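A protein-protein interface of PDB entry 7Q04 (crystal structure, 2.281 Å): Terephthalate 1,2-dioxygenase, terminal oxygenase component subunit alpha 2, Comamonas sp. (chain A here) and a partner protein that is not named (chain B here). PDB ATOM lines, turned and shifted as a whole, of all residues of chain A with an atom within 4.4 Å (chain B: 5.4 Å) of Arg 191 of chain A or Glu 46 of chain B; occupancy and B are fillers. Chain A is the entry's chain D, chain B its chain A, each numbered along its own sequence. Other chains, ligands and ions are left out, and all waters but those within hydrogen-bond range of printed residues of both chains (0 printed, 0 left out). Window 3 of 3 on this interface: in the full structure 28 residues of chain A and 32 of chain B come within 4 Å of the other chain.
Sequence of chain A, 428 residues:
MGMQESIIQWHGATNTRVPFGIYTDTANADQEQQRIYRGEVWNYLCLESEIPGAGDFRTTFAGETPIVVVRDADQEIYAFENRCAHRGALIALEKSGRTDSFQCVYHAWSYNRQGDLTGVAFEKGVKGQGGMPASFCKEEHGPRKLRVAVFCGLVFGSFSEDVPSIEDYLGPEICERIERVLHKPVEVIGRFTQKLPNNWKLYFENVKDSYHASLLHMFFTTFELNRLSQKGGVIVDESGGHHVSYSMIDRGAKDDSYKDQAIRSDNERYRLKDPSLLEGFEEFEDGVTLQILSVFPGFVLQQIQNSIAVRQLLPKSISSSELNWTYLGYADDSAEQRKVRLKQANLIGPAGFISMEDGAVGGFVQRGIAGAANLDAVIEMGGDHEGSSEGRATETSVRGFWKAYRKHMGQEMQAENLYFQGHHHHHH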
ATOM      1  N   GLU A  50      11.802 -18.046  -0.399  1.00  0.00           N
ATOM      2  CA  GLU A  50      12.890 -17.779   0.577  1.00  0.00           C
ATOM      3  C   GLU A  50      12.436 -16.764   1.644  1.00  0.00           C
ATOM      4  O   GLU A  50      13.115 -16.658   2.653  1.00  0.00           O
ATOM      5  CB  GLU A  50      14.145 -17.253  -0.116  1.00  0.00           C
ATOM      6  CG  GLU A  50      14.847 -18.269  -1.008  1.00  0.00           C
ATOM      7  CD  GLU A  50      16.113 -17.712  -1.646  1.00  0.00           C
ATOM      8  OE1 GLU A  50      16.052 -17.125  -2.752  1.00  0.00           O
ATOM      9  OE2 GLU A  50      17.156 -17.813  -0.987  1.00  0.00           O
ATOM     10  N   ARG A  58      15.683 -10.855   3.597  1.00  0.00           N
ATOM     11  CA  ARG A  58      17.058 -11.180   3.149  1.00  0.00           C
ATOM     12  C   ARG A  58      17.734  -9.854   2.790  1.00  0.00           C
ATOM     13  O   ARG A  58      16.993  -8.864   2.577  1.00  0.00           O
ATOM     14  CB  ARG A  58      17.034 -12.159   1.968  1.00  0.00           C
ATOM     15  CG  ARG A  58      16.564 -13.563   2.318  1.00  0.00           C
ATOM     16  CD  ARG A  58      16.826 -14.561   1.206  1.00  0.00           C
ATOM     17  NE  ARG A  58      18.186 -15.086   1.294  1.00  0.00           N
ATOM     18  CZ  ARG A  58      18.574 -16.106   2.060  1.00  0.00           C
ATOM     19  NH1 ARG A  58      19.840 -16.478   2.059  1.00  0.00           N
ATOM     20  NH2 ARG A  58      17.721 -16.752   2.831  1.00  0.00           N
ATOM     21  N   VAL A 188      14.256 -24.474  -2.070  1.00  0.00           N
ATOM     22  CA  VAL A 188      15.739 -24.339  -2.096  1.00  0.00           C
ATOM     23  C   VAL A 188      16.385 -25.602  -1.511  1.00  0.00           C
ATOM     24  O   VAL A 188      15.964 -26.003  -0.408  1.00  0.00           O
ATOM     25  CB  VAL A 188      16.195 -23.084  -1.344  1.00  0.00           C
ATOM     26  CG1 VAL A 188      17.710 -22.995  -1.349  1.00  0.00           C
ATOM     27  CG2 VAL A 188      15.594 -21.823  -1.944  1.00  0.00           C
ATOM     28  N   GLY A 190      20.029 -25.975  -1.752  1.00  0.00           N
ATOM     29  CA  GLY A 190      21.409 -25.576  -1.437  1.00  0.00           C
ATOM     30  C   GLY A 190      21.680 -24.193  -1.960  1.00  0.00           C
ATOM     31  O   GLY A 190      21.075 -23.841  -2.997  1.00  0.00           O
ATOM     32  N   ARG A 191      22.580 -23.463  -1.299  1.00  0.00           N
ATOM     33  CA  ARG A 191      23.206 -22.233  -1.847  1.00  0.00           C
ATOM     34  C   ARG A 191      24.722 -22.432  -1.880  1.00  0.00           C
ATOM     35  O   ARG A 191      25.237 -23.059  -0.944  1.00  0.00           O
ATOM     36  CB  ARG A 191      22.778 -21.033  -0.996  1.00  0.00           C
ATOM     37  CG  ARG A 191      21.325 -20.641  -1.228  1.00  0.00           C
ATOM     38  CD  ARG A 191      20.775 -19.486  -0.390  1.00  0.00           C
ATOM     39  NE  ARG A 191      20.246 -20.137   0.789  1.00  0.00           N
ATOM     40  CZ  ARG A 191      18.966 -20.192   1.168  1.00  0.00           C
ATOM     41  NH1 ARG A 191      18.001 -19.539   0.539  1.00  0.00           N
ATOM     42  NH2 ARG A 191      18.678 -20.893   2.243  1.00  0.00           N
ATOM     43  N   PHE A 192      25.380 -21.914  -2.918  1.00  0.00           N
ATOM     44  CA  PHE A 192      26.855 -21.799  -3.038  1.00  0.00           C
ATOM     45  C   PHE A 192      27.174 -20.503  -3.775  1.00  0.00           C
ATOM     46  O   PHE A 192      26.420 -20.106  -4.663  1.00  0.00           O
ATOM     47  CB  PHE A 192      27.461 -23.019  -3.724  1.00  0.00           C
ATOM     48  CG  PHE A 192      27.160 -24.318  -3.012  1.00  0.00           C
ATOM     49  CD1 PHE A 192      27.858 -24.689  -1.868  1.00  0.00           C
ATOM     50  CD2 PHE A 192      26.120 -25.132  -3.431  1.00  0.00           C
ATOM     51  CE1 PHE A 192      27.551 -25.860  -1.188  1.00  0.00           C
ATOM     52  CE2 PHE A 192      25.816 -26.308  -2.751  1.00  0.00           C
ATOM     53  CZ  PHE A 192      26.532 -26.674  -1.628  1.00  0.00           C
ATOM     54  N   TRP A 325      24.562 -19.094  -6.468  1.00  0.00           N
ATOM     55  CA  TRP A 325      23.753 -20.240  -6.918  1.00  0.00           C
ATOM     56  C   TRP A 325      22.653 -20.458  -5.884  1.00  0.00           C
ATOM     57  O   TRP A 325      22.973 -20.474  -4.679  1.00  0.00           O
ATOM     58  CB  TRP A 325      24.585 -21.513  -7.075  1.00  0.00           C
ATOM     59  CG  TRP A 325      25.597 -21.493  -8.177  1.00  0.00           C
ATOM     60  CD1 TRP A 325      26.865 -20.982  -8.114  1.00  0.00           C
ATOM     61  CD2 TRP A 325      25.460 -22.039  -9.492  1.00  0.00           C
ATOM     62  NE1 TRP A 325      27.521 -21.157  -9.299  1.00  0.00           N
ATOM     63  CE2 TRP A 325      26.682 -21.788 -10.173  1.00  0.00           C
ATOM     64  CE3 TRP A 325      24.429 -22.664 -10.184  1.00  0.00           C
ATOM     65  CZ2 TRP A 325      26.911 -22.196 -11.487  1.00  0.00           C
ATOM     66  CZ3 TRP A 325      24.655 -23.051 -11.494  1.00  0.00           C
ATOM     67  CH2 TRP A 325      25.881 -22.825 -12.137  1.00  0.00           C
ATOM     68  N   ASN B  40      28.474 -26.226   3.063  1.00  0.00           N
ATOM     69  CA  ASN B  40      28.881 -25.149   3.985  1.00  0.00           C
ATOM     70  C   ASN B  40      27.962 -25.133   5.203  1.00  0.00           C
ATOM     71  O   ASN B  40      26.993 -25.867   5.262  1.00  0.00           O
ATOM     72  CB  ASN B  40      28.923 -23.782   3.299  1.00  0.00           C
ATOM     73  CG  ASN B  40      27.645 -23.446   2.578  1.00  0.00           C
ATOM     74  OD1 ASN B  40      26.583 -23.591   3.164  1.00  0.00           O
ATOM     75  ND2 ASN B  40      27.761 -23.017   1.328  1.00  0.00           N
ATOM     76  N   VAL B  41      28.345 -24.328   6.169  1.00  0.00           N
ATOM     77  CA  VAL B  41      27.691 -24.223   7.491  1.00  0.00           C
ATOM     78  C   VAL B  41      26.252 -23.754   7.309  1.00  0.00           C
ATOM     79  O   VAL B  41      25.430 -24.201   8.090  1.00  0.00           O
ATOM     80  CB  VAL B  41      28.450 -23.235   8.387  1.00  0.00           C
ATOM     81  CG1 VAL B  41      29.781 -23.820   8.827  1.00  0.00           C
ATOM     82  CG2 VAL B  41      28.635 -21.888   7.695  1.00  0.00           C
ATOM     83  N   ASP B  42      25.982 -22.883   6.342  1.00  0.00           N
ATOM     84  CA  ASP B  42      24.618 -22.349   6.099  1.00  0.00           C
ATOM     85  C   ASP B  42      23.725 -23.523   5.695  1.00  0.00           C
ATOM     86  O   ASP B  42      22.687 -23.733   6.325  1.00  0.00           O
ATOM     87  CB  ASP B  42      24.586 -21.245   5.029  1.00  0.00           C
ATOM     88  CG  ASP B  42      25.056 -19.889   5.499  1.00  0.00           C
ATOM     89  OD1 ASP B  42      25.597 -19.788   6.658  1.00  0.00           O
ATOM     90  OD2 ASP B  42      24.860 -18.932   4.707  1.00  0.00           O
ATOM     91  N   ASN B  43      24.132 -24.268   4.683  1.00  0.00           N
ATOM     92  CA  ASN B  43      23.330 -25.402   4.184  1.00  0.00           C
ATOM     93  C   ASN B  43      23.182 -26.418   5.312  1.00  0.00           C
ATOM     94  O   ASN B  43      22.070 -26.978   5.461  1.00  0.00           O
ATOM     95  CB  ASN B  43      23.975 -26.064   2.983  1.00  0.00           C
ATOM     96  CG  ASN B  43      24.040 -25.144   1.785  1.00  0.00           C
ATOM     97  OD1 ASN B  43      23.184 -24.257   1.625  1.00  0.00           O
ATOM     98  ND2 ASN B  43      25.055 -25.358   0.944  1.00  0.00           N
ATOM     99  N   HIS B  44      24.263 -26.707   6.039  1.00  0.00           N
ATOM    100  CA  HIS B  44      24.253 -27.755   7.097  1.00  0.00           C
ATOM    101  C   HIS B  44      23.287 -27.341   8.231  1.00  0.00           C
ATOM    102  O   HIS B  44      22.542 -28.189   8.738  1.00  0.00           O
ATOM    103  CB  HIS B  44      25.669 -28.026   7.595  1.00  0.00           C
ATOM    104  CG  HIS B  44      25.744 -29.208   8.503  1.00  0.00           C
ATOM    105  ND1 HIS B  44      26.076 -29.096   9.854  1.00  0.00           N
ATOM    106  CD2 HIS B  44      25.590 -30.525   8.254  1.00  0.00           C
ATOM    107  CE1 HIS B  44      26.086 -30.283  10.417  1.00  0.00           C
ATOM    108  NE2 HIS B  44      25.813 -31.182   9.448  1.00  0.00           N
ATOM    109  N   ALA B  45      23.281 -26.060   8.588  1.00  0.00           N
ATOM    110  CA  ALA B  45      22.397 -25.484   9.633  1.00  0.00           C
ATOM    111  C   ALA B  45      20.928 -25.556   9.208  1.00  0.00           C
ATOM    112  O   ALA B  45      20.120 -25.951  10.055  1.00  0.00           O
ATOM    113  CB  ALA B  45      22.776 -24.063   9.963  1.00  0.00           C
ATOM    114  N   GLU B  46      20.584 -25.165   7.976  1.00  0.00           N
ATOM    115  CA  GLU B  46      19.192 -25.212   7.473  1.00  0.00           C
ATOM    116  C   GLU B  46      18.763 -26.600   6.983  1.00  0.00           C
ATOM    117  O   GLU B  46      17.630 -26.673   6.524  1.00  0.00           O
ATOM    118  CB  GLU B  46      19.015 -24.223   6.331  1.00  0.00           C
ATOM    119  CG  GLU B  46      19.263 -22.783   6.752  1.00  0.00           C
ATOM    120  CD  GLU B  46      19.337 -21.837   5.564  1.00  0.00           C
ATOM    121  OE1 GLU B  46      20.419 -21.149   5.404  1.00  0.00           O
ATOM    122  OE2 GLU B  46      18.327 -21.823   4.778  1.00  0.00           O
ATOM    123  N   GLY B  47      19.595 -27.641   7.058  1.00  0.00           N
ATOM    124  CA  GLY B  47      19.218 -29.016   6.675  1.00  0.00           C
ATOM    125  C   GLY B  47      19.229 -29.256   5.170  1.00  0.00           C
ATOM    126  O   GLY B  47      18.696 -30.245   4.778  1.00  0.00           O
ATOM    127  N   LEU B  48      19.847 -28.382   4.363  1.00  0.00           N
ATOM    128  CA  LEU B  48      19.888 -28.456   2.870  1.00  0.00           C
ATOM    129  C   LEU B  48      20.915 -29.496   2.438  1.00  0.00           C
ATOM    130  O   LEU B  48      22.011 -29.477   2.953  1.00  0.00           O
ATOM    131  CB  LEU B  48      20.221 -27.090   2.273  1.00  0.00           C
ATOM    132  CG  LEU B  48      19.358 -25.938   2.781  1.00  0.00           C
ATOM    133  CD1 LEU B  48      19.796 -24.606   2.213  1.00  0.00           C
ATOM    134  CD2 LEU B  48      17.891 -26.237   2.502  1.00  0.00           C
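Printed residues of chain B that touch a printed residue of chain A: Asn 40, Asn 43, Glu 46 and Leu 48. Hydrophobic or aromatic side chains of chain B within 4 Å of the printed part of chain A: Leu 48. Among the printed residues, 8 pairs touch across the chains.
The side-chain amide nitrogen of Asn 40 of chain B is in hydrogen-bond range of the backbone carbonyl oxygen of Arg 191 of chain A, at 3.4 Å. ND2 of Asn 43 of chain B is in hydrogen-bond range of O of Arg 191 of chain A. The side-chain carboxylate of Glu 46 of chain B is in salt-bridge range of the guanidinium group of Arg 191 of chain A, 2.7 Å away.
N of Asp 42 of chain B sits close to OD1 of Asn 40 of chain B, at 3.3 Å. The backbone NH (N) of Asn 43 of chain B sits at hydrogen-bond distance from the side-chain amide oxygen (OD1) of Asn 40 of chain B (3.0 Å). O of Asn 43 of chain B is in hydrogen-bond range of N of Leu 48 of chain B. The side-chain carboxylate (OE2) of Glu 50 of chain A is in salt-bridge range of the guanidinium group (NH1) of Arg 191 of chain A (2.5 Å). O of Phe 192 of chain A is in hydrogen-bond range of N of Trp 325 of chain A (2.8 Å).
Arg 191 of chain A touches just these residues of chain B: Asn 40 (3.4 Å), Asn 43 (3.0 Å), Glu 46 (2.7 Å) and Leu 48 (3.9 Å). Printed residues of chain B within 4 Å of Val 188 of chain A: Leu 48 (3.5 Å). Of the printed residues of chain B, Phe 192 of chain A touches Asn 40 (3.6 Å) and Asn 43 (3.2 Å).
Among the printed residues, merely in contact across the chains: Phe 192 of chain A with Asn 43 of chain B (3.2 Å), Val 188 of chain A with Leu 48 of chain B (3.5 Å), Phe 192 of chain A with Asn 40 of chain B (3.6 Å), Gly 190 of chain A with Asn 43 of chain B (3.8 Å) and Arg 191 of chain A with Leu 48 of chain B (3.9 Å).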
